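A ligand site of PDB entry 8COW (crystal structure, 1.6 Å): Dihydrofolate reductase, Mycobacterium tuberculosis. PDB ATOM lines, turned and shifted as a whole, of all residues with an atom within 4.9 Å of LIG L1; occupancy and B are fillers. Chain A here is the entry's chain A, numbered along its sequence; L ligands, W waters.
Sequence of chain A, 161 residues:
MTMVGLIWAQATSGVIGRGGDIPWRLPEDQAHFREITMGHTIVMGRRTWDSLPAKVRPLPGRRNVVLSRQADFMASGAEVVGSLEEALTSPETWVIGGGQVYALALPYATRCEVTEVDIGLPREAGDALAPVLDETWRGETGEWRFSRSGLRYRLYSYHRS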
ATOM      1  N   ILE A   7      20.496 -20.870 -10.617  1.00  0.00           N
ATOM      2  CA  ILE A   7      20.845 -21.823  -9.572  1.00  0.00           C
ATOM      3  C   ILE A   7      19.558 -22.481  -9.068  1.00  0.00           C
ATOM      4  O   ILE A   7      18.585 -21.780  -8.730  1.00  0.00           O
ATOM      5  CB  ILE A   7      21.642 -21.144  -8.433  1.00  0.00           C
ATOM      6  CG1 ILE A   7      22.108 -22.157  -7.381  1.00  0.00           C
ATOM      7  CG2 ILE A   7      20.849 -20.000  -7.778  1.00  0.00           C
ATOM      8  CD1 ILE A   7      23.374 -21.682  -6.603  1.00  0.00           C
ATOM      9  N   TRP A   8      19.537 -23.808  -9.019  1.00  0.00           N
ATOM     10  CA  TRP A   8      18.373 -24.516  -8.487  1.00  0.00           C
ATOM     11  C   TRP A   8      18.780 -25.868  -7.919  1.00  0.00           C
ATOM     12  O   TRP A   8      19.852 -26.398  -8.221  1.00  0.00           O
ATOM     13  CB  TRP A   8      17.296 -24.705  -9.567  1.00  0.00           C
ATOM     14  CG  TRP A   8      17.608 -25.707 -10.638  1.00  0.00           C
ATOM     15  CD1 TRP A   8      17.487 -27.068 -10.569  1.00  0.00           C
ATOM     16  CD2 TRP A   8      18.048 -25.407 -11.965  1.00  0.00           C
ATOM     17  NE1 TRP A   8      17.830 -27.621 -11.782  1.00  0.00           N
ATOM     18  CE2 TRP A   8      18.184 -26.626 -12.654  1.00  0.00           C
ATOM     19  CE3 TRP A   8      18.357 -24.211 -12.629  1.00  0.00           C
ATOM     20  CZ2 TRP A   8      18.611 -26.692 -13.976  1.00  0.00           C
ATOM     21  CZ3 TRP A   8      18.773 -24.284 -13.944  1.00  0.00           C
ATOM     22  CH2 TRP A   8      18.888 -25.516 -14.606  1.00  0.00           C
ATOM     23  N   ALA A   9      17.892 -26.430  -7.109  1.00  0.00           N
ATOM     24  CA  ALA A   9      18.033 -27.785  -6.605  1.00  0.00           C
ATOM     25  C   ALA A   9      16.810 -28.579  -7.046  1.00  0.00           C
ATOM     26  O   ALA A   9      15.678 -28.144  -6.835  1.00  0.00           O
ATOM     27  CB  ALA A   9      18.168 -27.803  -5.085  1.00  0.00           C
ATOM     28  N   ILE A  16      11.173 -29.127  -8.630  1.00  0.00           N
ATOM     29  CA  ILE A  16      11.829 -28.207  -7.703  1.00  0.00           C
ATOM     30  C   ILE A  16      10.897 -27.681  -6.622  1.00  0.00           C
ATOM     31  O   ILE A  16      11.381 -27.153  -5.614  1.00  0.00           O
ATOM     32  CB  ILE A  16      12.487 -27.024  -8.478  1.00  0.00           C
ATOM     33  CG1 ILE A  16      11.429 -26.210  -9.226  1.00  0.00           C
ATOM     34  CG2 ILE A  16      13.520 -27.539  -9.482  1.00  0.00           C
ATOM     35  CD1 ILE A  16      11.931 -24.865  -9.688  1.00  0.00           C
ATOM     36  N   GLY A  17       9.583 -27.823  -6.769  1.00  0.00           N
ATOM     37  CA  GLY A  17       8.688 -27.228  -5.799  1.00  0.00           C
ATOM     38  C   GLY A  17       7.293 -27.796  -5.916  1.00  0.00           C
ATOM     39  O   GLY A  17       6.868 -28.234  -6.990  1.00  0.00           O
ATOM     40  N   ARG A  18       6.572 -27.776  -4.806  1.00  0.00           N
ATOM     41  CA  ARG A  18       5.212 -28.278  -4.768  1.00  0.00           C
ATOM     42  C   ARG A  18       4.460 -27.586  -3.639  1.00  0.00           C
ATOM     43  O   ARG A  18       4.977 -27.499  -2.520  1.00  0.00           O
ATOM     44  CB  ARG A  18       5.204 -29.798  -4.566  1.00  0.00           C
ATOM     45  CG  ARG A  18       3.837 -30.459  -4.589  1.00  0.00           C
ATOM     46  CD  ARG A  18       4.074 -31.943  -4.438  1.00  0.00           C
ATOM     47  NE  ARG A  18       4.563 -32.507  -5.680  1.00  0.00           N
ATOM     48  CZ  ARG A  18       5.032 -33.740  -5.743  1.00  0.00           C
ATOM     49  NH1 ARG A  18       5.122 -34.428  -4.625  1.00  0.00           N
ATOM     50  NH2 ARG A  18       5.453 -34.255  -6.884  1.00  0.00           N
ATOM     51  N   GLY A  20       3.880 -24.563  -2.921  1.00  0.00           N
ATOM     52  CA  GLY A  20       4.545 -23.398  -2.373  1.00  0.00           C
ATOM     53  C   GLY A  20       5.751 -23.705  -1.513  1.00  0.00           C
ATOM     54  O   GLY A  20       6.221 -22.820  -0.785  1.00  0.00           O
ATOM     55  N   ASP A  21       6.259 -24.940  -1.563  1.00  0.00           N
ATOM     56  CA  ASP A  21       7.281 -25.406  -0.644  1.00  0.00           C
ATOM     57  C   ASP A  21       8.316 -26.187  -1.438  1.00  0.00           C
ATOM     58  O   ASP A  21       8.104 -26.505  -2.614  1.00  0.00           O
ATOM     59  CB  ASP A  21       6.665 -26.280   0.453  1.00  0.00           C
ATOM     60  CG  ASP A  21       7.680 -26.731   1.498  1.00  0.00           C
ATOM     61  OD1 ASP A  21       8.542 -25.924   1.898  1.00  0.00           O
ATOM     62  OD2 ASP A  21       7.606 -27.919   1.883  1.00  0.00           O
ATOM     63  N   ILE A  22       9.447 -26.487  -0.804  1.00  0.00           N
ATOM     64  CA  ILE A  22      10.438 -27.375  -1.391  1.00  0.00           C
ATOM     65  C   ILE A  22      10.406 -28.678  -0.585  1.00  0.00           C
ATOM     66  O   ILE A  22      10.781 -28.667   0.596  1.00  0.00           O
ATOM     67  CB  ILE A  22      11.834 -26.740  -1.426  1.00  0.00           C
ATOM     68  CG1 ILE A  22      11.808 -25.493  -2.290  1.00  0.00           C
ATOM     69  CG2 ILE A  22      12.892 -27.719  -1.979  1.00  0.00           C
ATOM     70  CD1 ILE A  22      13.061 -24.631  -2.176  1.00  0.00           C
ATOM     71  N   TRP A  24      11.875 -31.279   0.566  1.00  0.00           N
ATOM     72  CA  TRP A  24      13.009 -31.981   1.175  1.00  0.00           C
ATOM     73  C   TRP A  24      13.787 -30.976   2.022  1.00  0.00           C
ATOM     74  O   TRP A  24      13.489 -29.776   2.039  1.00  0.00           O
ATOM     75  CB  TRP A  24      13.938 -32.638   0.144  1.00  0.00           C
ATOM     76  CG  TRP A  24      14.557 -31.659  -0.807  1.00  0.00           C
ATOM     77  CD1 TRP A  24      15.620 -30.843  -0.582  1.00  0.00           C
ATOM     78  CD2 TRP A  24      14.133 -31.395  -2.155  1.00  0.00           C
ATOM     79  NE1 TRP A  24      15.889 -30.089  -1.710  1.00  0.00           N
ATOM     80  CE2 TRP A  24      14.984 -30.400  -2.690  1.00  0.00           C
ATOM     81  CE3 TRP A  24      13.107 -31.896  -2.971  1.00  0.00           C
ATOM     82  CZ2 TRP A  24      14.853 -29.902  -3.984  1.00  0.00           C
ATOM     83  CZ3 TRP A  24      12.976 -31.405  -4.257  1.00  0.00           C
ATOM     84  CH2 TRP A  24      13.845 -30.419  -4.760  1.00  0.00           C
ATOM     85  N   GLY A  45      10.848 -15.062  -8.753  1.00  0.00           N
ATOM     86  CA  GLY A  45       9.444 -14.839  -9.062  1.00  0.00           C
ATOM     87  C   GLY A  45       8.637 -14.525  -7.826  1.00  0.00           C
ATOM     88  O   GLY A  45       9.030 -14.813  -6.701  1.00  0.00           O
ATOM     89  N   ARG A  46       7.484 -13.882  -8.050  1.00  0.00           N
ATOM     90  CA  ARG A  46       6.666 -13.433  -6.924  1.00  0.00           C
ATOM     91  C   ARG A  46       6.255 -14.600  -6.025  1.00  0.00           C
ATOM     92  O   ARG A  46       6.259 -14.480  -4.796  1.00  0.00           O
ATOM     93  CB  ARG A  46       5.434 -12.670  -7.438  1.00  0.00           C
ATOM     94  CG  ARG A  46       4.658 -11.854  -6.391  1.00  0.00           C
ATOM     95  CD  ARG A  46       3.499 -12.669  -5.802  1.00  0.00           C
ATOM     96  NE  ARG A  46       2.649 -13.241  -6.845  1.00  0.00           N
ATOM     97  CZ  ARG A  46       1.833 -14.277  -6.660  1.00  0.00           C
ATOM     98  NH1 ARG A  46       1.765 -14.878  -5.480  1.00  0.00           N
ATOM     99  NH2 ARG A  46       1.110 -14.754  -7.661  1.00  0.00           N
ATOM    100  N   ARG A  47       5.930 -15.757  -6.630  1.00  0.00           N
ATOM    101  CA  ARG A  47       5.516 -16.900  -5.814  1.00  0.00           C
ATOM    102  C   ARG A  47       6.656 -17.381  -4.928  1.00  0.00           C
ATOM    103  O   ARG A  47       6.427 -17.831  -3.801  1.00  0.00           O
ATOM    104  CB  ARG A  47       5.020 -18.043  -6.694  1.00  0.00           C
ATOM    105  CG  ARG A  47       3.829 -17.690  -7.543  1.00  0.00           C
ATOM    106  CD  ARG A  47       2.970 -18.908  -7.860  1.00  0.00           C
ATOM    107  NE  ARG A  47       2.497 -18.829  -9.230  1.00  0.00           N
ATOM    108  CZ  ARG A  47       1.243 -18.554  -9.569  1.00  0.00           C
ATOM    109  NH1 ARG A  47       0.354 -18.290  -8.617  1.00  0.00           N
ATOM    110  NH2 ARG A  47       0.892 -18.482 -10.850  1.00  0.00           N
ATOM    111  N   THR A  48       7.898 -17.289  -5.408  1.00  0.00           N
ATOM    112  CA  THR A  48       9.025 -17.686  -4.584  1.00  0.00           C
ATOM    113  C   THR A  48       9.264 -16.679  -3.463  1.00  0.00           C
ATOM    114  O   THR A  48       9.522 -17.062  -2.316  1.00  0.00           O
ATOM    115  CB  THR A  48      10.261 -17.873  -5.449  1.00  0.00           C
ATOM    116  OG1 THR A  48      10.054 -19.007  -6.300  1.00  0.00           O
ATOM    117  CG2 THR A  48      11.482 -18.136  -4.592  1.00  0.00           C
ATOM    118  N   SER A  51       6.920 -17.410  -0.814  1.00  0.00           N
ATOM    119  CA  SER A  51       7.219 -18.625  -0.054  1.00  0.00           C
ATOM    120  C   SER A  51       8.248 -18.387   1.051  1.00  0.00           C
ATOM    121  O   SER A  51       8.408 -19.265   1.919  1.00  0.00           O
ATOM    122  CB  SER A  51       7.728 -19.736  -0.986  1.00  0.00           C
ATOM    123  OG  SER A  51       9.062 -19.502  -1.428  1.00  0.00           O
ATOM    124  N   LEU A  67      10.217 -10.496  -9.547  1.00  0.00           N
ATOM    125  CA  LEU A  67       9.419 -10.372 -10.778  1.00  0.00           C
ATOM    126  C   LEU A  67       7.930 -10.571 -10.518  1.00  0.00           C
ATOM    127  O   LEU A  67       7.503 -11.640 -10.078  1.00  0.00           O
ATOM    128  CB  LEU A  67       9.840 -11.371 -11.843  1.00  0.00           C
ATOM    129  CG  LEU A  67      11.034 -11.120 -12.735  1.00  0.00           C
ATOM    130  CD1 LEU A  67      11.194 -12.316 -13.646  1.00  0.00           C
ATOM    131  CD2 LEU A  67      10.702  -9.889 -13.573  1.00  0.00           C
ATOM    132  N   SER A  68       7.136  -9.582 -10.915  1.00  0.00           N
ATOM    133  CA  SER A  68       5.690  -9.708 -10.903  1.00  0.00           C
ATOM    134  C   SER A  68       5.119  -8.925 -12.065  1.00  0.00           C
ATOM    135  O   SER A  68       5.705  -7.920 -12.499  1.00  0.00           O
ATOM    136  CB  SER A  68       5.106  -9.193  -9.588  1.00  0.00           C
ATOM    137  OG  SER A  68       3.699  -9.098  -9.668  1.00  0.00           O
ATOM    138  N   ARG A  69       3.967  -9.367 -12.545  1.00  0.00           N
ATOM    139  CA  ARG A  69       3.217  -8.560 -13.503  1.00  0.00           C
ATOM    140  C   ARG A  69       2.294  -7.547 -12.828  1.00  0.00           C
ATOM    141  O   ARG A  69       1.694  -6.723 -13.525  1.00  0.00           O
ATOM    142  CB  ARG A  69       2.384  -9.456 -14.406  1.00  0.00           C
ATOM    143  CG  ARG A  69       3.204 -10.491 -15.127  1.00  0.00           C
ATOM    144  CD  ARG A  69       2.400 -11.170 -16.202  1.00  0.00           C
ATOM    145  NE  ARG A  69       3.289 -11.801 -17.176  1.00  0.00           N
ATOM    146  CZ  ARG A  69       3.766 -13.044 -17.043  1.00  0.00           C
ATOM    147  NH1 ARG A  69       3.452 -13.768 -15.981  1.00  0.00           N
ATOM    148  NH2 ARG A  69       4.575 -13.534 -17.972  1.00  0.00           N
ATOM    149  N   GLN A  70       2.155  -7.615 -11.511  1.00  0.00           N
ATOM    150  CA  GLN A  70       1.377  -6.643 -10.748  1.00  0.00           C
ATOM    151  C   GLN A  70       2.113  -5.311 -10.690  1.00  0.00           C
ATOM    152  O   GLN A  70       3.145  -5.199 -10.016  1.00  0.00           O
ATOM    153  CB  GLN A  70       1.133  -7.173  -9.341  1.00  0.00           C
ATOM    154  CG  GLN A  70       0.293  -8.427  -9.278  1.00  0.00           C
ATOM    155  CD  GLN A  70       0.046  -8.854  -7.840  1.00  0.00           C
ATOM    156  OE1 GLN A  70      -0.613  -8.157  -7.073  1.00  0.00           O
ATOM    157  NE2 GLN A  70       0.570 -10.035  -7.478  1.00  0.00           N
ATOM    158  N   GLY A  82       8.951  -5.524 -13.535  1.00  0.00           N
ATOM    159  CA  GLY A  82       7.940  -6.142 -14.378  1.00  0.00           C
ATOM    160  C   GLY A  82       8.456  -6.985 -15.520  1.00  0.00           C
ATOM    161  O   GLY A  82       7.653  -7.630 -16.211  1.00  0.00           O
ATOM    162  N   SER A  83       9.762  -7.001 -15.764  1.00  0.00           N
ATOM    163  CA  SER A  83      10.299  -7.904 -16.774  1.00  0.00           C
ATOM    164  C   SER A  83      11.668  -8.355 -16.315  1.00  0.00           C
ATOM    165  O   SER A  83      12.369  -7.636 -15.595  1.00  0.00           O
ATOM    166  CB  SER A  83      10.444  -7.236 -18.153  1.00  0.00           C
ATOM    167  OG  SER A  83      11.401  -6.203 -18.068  1.00  0.00           O
ATOM    168  N   ILE A  96      17.129 -17.230  -8.955  1.00  0.00           N
ATOM    169  CA  ILE A  96      17.043 -18.217  -7.877  1.00  0.00           C
ATOM    170  C   ILE A  96      15.677 -18.901  -7.804  1.00  0.00           C
ATOM    171  O   ILE A  96      15.412 -19.616  -6.823  1.00  0.00           O
ATOM    172  CB  ILE A  96      17.426 -17.611  -6.519  1.00  0.00           C
ATOM    173  CG1 ILE A  96      16.382 -16.596  -6.025  1.00  0.00           C
ATOM    174  CG2 ILE A  96      18.818 -16.950  -6.621  1.00  0.00           C
ATOM    175  CD1 ILE A  96      16.436 -16.294  -4.524  1.00  0.00           C
ATOM    176  N   GLY A  97      14.816 -18.731  -8.797  1.00  0.00           N
ATOM    177  CA  GLY A  97      13.578 -19.481  -8.887  1.00  0.00           C
ATOM    178  C   GLY A  97      12.359 -18.562  -8.972  1.00  0.00           C
ATOM    179  O   GLY A  97      12.461 -17.349  -8.840  1.00  0.00           O
ATOM    180  N   GLY A  98      11.192 -19.184  -9.175  1.00  0.00           N
ATOM    181  CA  GLY A  98      11.027 -20.629  -9.339  1.00  0.00           C
ATOM    182  C   GLY A  98      10.895 -21.117 -10.786  1.00  0.00           C
ATOM    183  O   GLY A  98      11.586 -20.624 -11.671  1.00  0.00           O
ATOM    184  N   GLY A  99      10.010 -22.078 -11.027  1.00  0.00           N
ATOM    185  CA  GLY A  99       9.959 -22.714 -12.346  1.00  0.00           C
ATOM    186  C   GLY A  99       9.676 -21.729 -13.465  1.00  0.00           C
ATOM    187  O   GLY A  99      10.295 -21.788 -14.533  1.00  0.00           O
ATOM    188  N   GLN A 100       8.709 -20.836 -13.256  1.00  0.00           N
ATOM    189  CA  GLN A 100       8.361 -19.885 -14.315  1.00  0.00           C
ATOM    190  C   GLN A 100       9.516 -18.962 -14.615  1.00  0.00           C
ATOM    191  O   GLN A 100       9.818 -18.682 -15.785  1.00  0.00           O
ATOM    192  CB  GLN A 100       7.109 -19.087 -13.924  1.00  0.00           C
ATOM    193  CG  GLN A 100       5.853 -19.922 -13.877  1.00  0.00           C
ATOM    194  CD  GLN A 100       4.586 -19.086 -13.737  1.00  0.00           C
ATOM    195  OE1 GLN A 100       4.644 -17.850 -13.677  1.00  0.00           O
ATOM    196  NE2 GLN A 100       3.442 -19.744 -13.674  1.00  0.00           N
ATOM    197  N   VAL A 101      10.204 -18.477 -13.583  1.00  0.00           N
ATOM    198  CA  VAL A 101      11.283 -17.514 -13.790  1.00  0.00           C
ATOM    199  C   VAL A 101      12.510 -18.185 -14.414  1.00  0.00           C
ATOM    200  O   VAL A 101      13.201 -17.563 -15.236  1.00  0.00           O
ATOM    201  CB  VAL A 101      11.619 -16.775 -12.482  1.00  0.00           C
ATOM    202  CG1 VAL A 101      12.885 -15.950 -12.613  1.00  0.00           C
ATOM    203  CG2 VAL A 101      10.477 -15.849 -12.113  1.00  0.00           C
ATOM    204  N   TYR A 102      12.810 -19.445 -14.058  1.00  0.00           N
ATOM    205  CA  TYR A 102      13.940 -20.134 -14.700  1.00  0.00           C
ATOM    206  C   TYR A 102      13.723 -20.236 -16.202  1.00  0.00           C
ATOM    207  O   TYR A 102      14.657 -20.039 -16.993  1.00  0.00           O
ATOM    208  CB  TYR A 102      14.090 -21.545 -14.138  1.00  0.00           C
ATOM    209  CG  TYR A 102      14.613 -21.645 -12.745  1.00  0.00           C
ATOM    210  CD1 TYR A 102      15.675 -20.866 -12.308  1.00  0.00           C
ATOM    211  CD2 TYR A 102      14.029 -22.519 -11.838  1.00  0.00           C
ATOM    212  CE1 TYR A 102      16.136 -20.965 -10.981  1.00  0.00           C
ATOM    213  CE2 TYR A 102      14.491 -22.626 -10.516  1.00  0.00           C
ATOM    214  CZ  TYR A 102      15.545 -21.843 -10.103  1.00  0.00           C
ATOM    215  OH  TYR A 102      15.977 -21.953  -8.785  1.00  0.00           O
ATOM    216  N   LEU A 104      11.979 -18.339 -18.083  1.00  0.00           N
ATOM    217  CA  LEU A 104      12.065 -17.013 -18.691  1.00  0.00           C
ATOM    218  C   LEU A 104      13.513 -16.585 -18.810  1.00  0.00           C
ATOM    219  O   LEU A 104      13.891 -15.894 -19.780  1.00  0.00           O
ATOM    220  CB  LEU A 104      11.273 -16.015 -17.832  1.00  0.00           C
ATOM    221  CG  LEU A 104      11.229 -14.539 -18.237  1.00  0.00           C
ATOM    222  CD1 LEU A 104      10.521 -14.378 -19.576  1.00  0.00           C
ATOM    223  CD2 LEU A 104      10.620 -13.611 -17.146  1.00  0.00           C
ATOM    224  N   ALA A 128       6.288 -27.293  -9.837  1.00  0.00           N
ATOM    225  CA  ALA A 128       7.299 -26.467 -10.460  1.00  0.00           C
ATOM    226  C   ALA A 128       8.483 -27.333 -10.895  1.00  0.00           C
ATOM    227  O   ALA A 128       8.924 -28.225 -10.168  1.00  0.00           O
ATOM    228  CB  ALA A 128       7.779 -25.390  -9.466  1.00  0.00           C
HETATM  229  P1  LIG L   1       7.752 -18.399  -9.613  1.00  0.00           P
HETATM  230  O1  LIG L   1       8.555 -18.348  -8.409  1.00  0.00           O
HETATM  231  O2  LIG L   1       8.406 -18.586 -10.870  1.00  0.00           O
HETATM  232  O3  LIG L   1       6.864 -17.096  -9.663  1.00  0.00           O
HETATM  233  C1  LIG L   1       5.872 -16.964 -10.640  1.00  0.00           C
HETATM  234  C2  LIG L   1       5.456 -15.512 -10.697  1.00  0.00           C
HETATM  235  O4  LIG L   1       6.477 -14.718 -11.293  1.00  0.00           O
HETATM  236  C3  LIG L   1       4.214 -15.196 -11.512  1.00  0.00           C
HETATM  237  O5  LIG L   1       3.051 -15.551 -10.790  1.00  0.00           O
HETATM  238  C4  LIG L   1       4.397 -13.709 -11.709  1.00  0.00           C
HETATM  239  O6  LIG L   1       4.008 -13.032 -10.553  1.00  0.00           O
HETATM  240  C5  LIG L   1       5.903 -13.626 -11.932  1.00  0.00           C
HETATM  241  N1  LIG L   1       6.277 -13.683 -13.326  1.00  0.00           N
HETATM  242  C6  LIG L   1       6.261 -14.811 -14.088  1.00  0.00           C
HETATM  243  N2  LIG L   1       6.597 -14.594 -15.318  1.00  0.00           N
HETATM  244  C7  LIG L   1       6.831 -13.245 -15.393  1.00  0.00           C
HETATM  245  C8  LIG L   1       7.193 -12.395 -16.455  1.00  0.00           C
HETATM  246  N3  LIG L   1       7.373 -12.822 -17.689  1.00  0.00           N
HETATM  247  N4  LIG L   1       7.350 -11.082 -16.191  1.00  0.00           N
HETATM  248  C9  LIG L   1       7.149 -10.664 -14.952  1.00  0.00           C
HETATM  249  N5  LIG L   1       6.791 -11.362 -13.885  1.00  0.00           N
HETATM  250  C10 LIG L   1       6.635 -12.663 -14.165  1.00  0.00           C
HETATM  251  O7  LIG L   1       6.662 -19.515  -9.526  1.00  0.00           O
HETATM  252  P2  LIG L   1       6.700 -21.089  -9.671  1.00  0.00           P
HETATM  253  O8  LIG L   1       5.406 -21.539  -9.206  1.00  0.00           O
HETATM  254  O9  LIG L   1       7.091 -21.468 -11.012  1.00  0.00           O
HETATM  255  O10 LIG L   1       7.783 -21.579  -8.641  1.00  0.00           O
HETATM  256  C11 LIG L   1       7.545 -21.560  -7.246  1.00  0.00           C
HETATM  257  C12 LIG L   1       7.937 -22.860  -6.600  1.00  0.00           C
HETATM  258  O11 LIG L   1       9.322 -23.193  -6.812  1.00  0.00           O
HETATM  259  C13 LIG L   1       7.745 -22.936  -5.088  1.00  0.00           C
HETATM  260  O12 LIG L   1       7.283 -24.231  -4.762  1.00  0.00           O
HETATM  261  C14 LIG L   1       9.154 -22.741  -4.589  1.00  0.00           C
HETATM  262  O13 LIG L   1       9.341 -23.326  -3.349  1.00  0.00           O
HETATM  263  C15 LIG L   1       9.913 -23.526  -5.613  1.00  0.00           C
HETATM  264  N6  LIG L   1      11.337 -23.155  -5.649  1.00  0.00           N
HETATM  265  C16 LIG L   1      12.288 -24.114  -5.580  1.00  0.00           C
HETATM  266  C17 LIG L   1      13.563 -23.863  -5.794  1.00  0.00           C
HETATM  267  C18 LIG L   1      14.517 -24.954  -5.803  1.00  0.00           C
HETATM  268  O14 LIG L   1      14.195 -26.090  -5.513  1.00  0.00           O
HETATM  269  N7  LIG L   1      15.732 -24.600  -6.116  1.00  0.00           N
HETATM  270  C19 LIG L   1      13.991 -22.498  -5.988  1.00  0.00           C
HETATM  271  C20 LIG L   1      12.926 -21.513  -5.889  1.00  0.00           C
HETATM  272  C21 LIG L   1      11.689 -21.867  -5.730  1.00  0.00           C
HETATM  273  P3  LIG L   1       2.567 -12.328 -10.370  1.00  0.00           P
HETATM  274  O15 LIG L   1       1.657 -13.388 -10.309  1.00  0.00           O
HETATM  275  O16 LIG L   1       2.384 -11.507 -11.500  1.00  0.00           O
HETATM  276  O17 LIG L   1       2.653 -11.583  -9.181  1.00  0.00           O
HETATM  277  C1  LG2 L   2      16.611 -24.860  -1.435  1.00  0.00           C
HETATM  278  C2  LG2 L   2      14.442 -19.789  -2.932  1.00  0.00           C
HETATM  279  C3  LG2 L   2      14.735 -18.884  -1.749  1.00  0.00           C
HETATM  280  C4  LG2 L   2      19.620 -24.138  -4.729  1.00  0.00           C
HETATM  281  C5  LG2 L   2      18.058 -23.516  -3.023  1.00  0.00           C
HETATM  282  C6  LG2 L   2      17.559 -22.510  -3.878  1.00  0.00           C
HETATM  283  C7  LG2 L   2      18.191 -22.416  -5.106  1.00  0.00           C
HETATM  284  C8  LG2 L   2      17.516 -23.815  -1.609  1.00  0.00           C
HETATM  285  C9  LG2 L   2      17.937 -23.067  -0.521  1.00  0.00           C
HETATM  286  C10 LG2 L   2      17.441 -23.351   0.753  1.00  0.00           C
HETATM  287  C11 LG2 L   2      16.527 -24.391   0.919  1.00  0.00           C
HETATM  288  C12 LG2 L   2      16.107 -25.146  -0.176  1.00  0.00           C
HETATM  289  C13 LG2 L   2      16.442 -21.557  -3.487  1.00  0.00           C
HETATM  290  C14 LG2 L   2      15.565 -20.782  -3.253  1.00  0.00           C
HETATM  291  C15 LG2 L   2      13.763 -20.044  -1.592  1.00  0.00           C
HETATM  292  F1  LG2 L   2      18.835 -22.051  -0.693  1.00  0.00           F
HETATM  293  N1  LG2 L   2      19.172 -23.179  -5.543  1.00  0.00           N
HETATM  294  N2  LG2 L   2      19.034 -24.246  -3.537  1.00  0.00           N
HETATM  295  N3  LG2 L   2      17.726 -21.384  -6.017  1.00  0.00           N
HETATM  296  N4  LG2 L   2      20.709 -25.002  -5.140  1.00  0.00           N
HETATM  297  O   HOH W   1      -0.540 -10.413 -11.613  1.00  0.00           O
HETATM  298  O   HOH W   2       5.820 -23.418 -12.252  1.00  0.00           O
HETATM  299  O   HOH W   3       4.797 -24.758  -5.614  1.00  0.00           O
HETATM  300  O   HOH W   4       3.953 -22.792  -6.783  1.00  0.00           O
HETATM  301  O   HOH W   5      -1.150 -13.657 -10.817  1.00  0.00           O
HETATM  302  O   HOH W   6      10.569 -21.835  -1.860  1.00  0.00           O
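The backbone NH of Thr 48 sits at hydrogen-bond distance from an oxygen (O1) of LIG L1 (3.2 Å).
OG1 of Thr 48 lies within hydrogen-bond range of O1 of LIG L1 (2.7 Å).
N of Ser 68 sits close to N5 of LIG L1 (3.5 Å).
An oxygen (O17) of LIG L1 lies within hydrogen-bond range of the side-chain hydroxyl (OG) of Ser 68, 2.7 Å away.
The backbone NH of Gln 100 lies within hydrogen-bond range of an oxygen (O9) of LIG L1.
The backbone NH of Arg 69 lies within hydrogen-bond range of an oxygen (O16) of LIG L1, at 2.9 Å.
NH1 of Arg 69 sits at hydrogen-bond distance from N2 of LIG L1 (3.3 Å).
O4 of LIG L1 lies within hydrogen-bond range of N of Arg 46.
The guanidinium group (NE) of Arg 46 lies within salt-bridge range of an oxygen (O17) of LIG L1, at 2.9 Å.
The backbone NH of Gly 98 is in hydrogen-bond range of an oxygen (O1) of LIG L1 (2.9 Å).
The backbone NH (N) of Gly 99 sits at hydrogen-bond distance from an oxygen (O9) of LIG L1, at 3.0 Å.
NE2 of Gln 70 sits at hydrogen-bond distance from O17 of LIG L1, at 3.1 Å.
O12 of LIG L1 is in hydrogen-bond range of N of Asp 21 (3.4 Å).
The backbone carbonyl oxygen of Asp 21 is in hydrogen-bond range of an oxygen (O12) of LIG L1 (3.2 Å).
N of Val 101 is in hydrogen-bond range of O2 of LIG L1, 3.3 Å away.
The backbone NH of Arg 47 lies within hydrogen-bond range of an oxygen (O3) of LIG L1 (3.4 Å).
O8 of LIG L1 is in salt-bridge range of NE of Arg 47.
O of Ile 96 sits at hydrogen-bond distance from N3 of LG2 L2.
A nitrogen (N3) of LG2 L2 is in hydrogen-bond range of the side-chain hydroxyl (OH) of Tyr 102, 3.3 Å away.
O of Trp 8 sits at hydrogen-bond distance from N4 of LG2 L2, 3.5 Å away.
O of Ile 7 sits at hydrogen-bond distance from N3 of LG2 L2, 2.9 Å away.
N of Gly 98 lies within hydrogen-bond range of OG1 of Thr 48.
The backbone NH (N) of Gln 70 sits at hydrogen-bond distance from the side-chain hydroxyl (OG) of Ser 68 (2.8 Å).
The backbone carbonyl oxygen of Leu 67 sits at hydrogen-bond distance from the backbone NH of Arg 46, at 3.0 Å.
The backbone carbonyl oxygen of Ala 128 lies within hydrogen-bond range of the backbone NH of Ile 16, 2.9 Å away.
The side-chain hydroxyl of Tyr 102 lies within hydrogen-bond range of the backbone carbonyl oxygen of Ile 96, at 3.1 Å.
The backbone carbonyl oxygen (O) of Gly 17 lies within hydrogen-bond range of the backbone NH (N) of Ala 128 (3.1 Å).
OH of Tyr 102 sits close to N of Gly 97, at 3.4 Å.
O of Gly 97 lies within hydrogen-bond range of N of Gly 45, at 2.8 Å.
An oxygen (O14) of LIG L1 lies close to the backbone carbonyl oxygen (O) of Ala 9 (2.9 Å).
An oxygen (O14) of LIG L1 sits close to the backbone carbonyl oxygen (O) of Ile 16 (3.0 Å).
The backbone carbonyl oxygen (O) of Leu 67 lies close to an oxygen (O4) of LIG L1 (3.5 Å).
A nitrogen (N4) of LIG L1 sits close to the backbone carbonyl oxygen (O) of Gly 82.
CA of Trp 8 touches N7 of LIG L1 (3.6 Å).
Gly 17 touches LIG L1.
Arg 18 touches LIG L1 (N to O12, 3.6 Å).
Gly 20 touches LIG L1.
Ile 22 touches LIG L1 (CG1 to O13, 3.5 Å).
Gly 45 touches LIG L1 (CA to O3, 3.5 Å).
O of Ile 96 touches C20 of LIG L1, at 3.3 Å.
Gly 97 touches LIG L1.
Tyr 102 touches LIG L1.
Leu 104 touches LIG L1.
Ala 128 touches LIG L1.
Of the 30 residues printed, 26 come within 4 Å of LIG L1.
Along chain A the residues within 4 Å of LIG L1 span positions 8 to 128.
The nearest printed residue that does not touch LIG L1 is Trp 24 (4.2 Å).
Water W6 bridges O13 of LIG L1 (2.4 Å) and OG of Ser 51 (2.8 Å).
Water W3 bridges O12 of LIG L1 and N of Gly 20.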
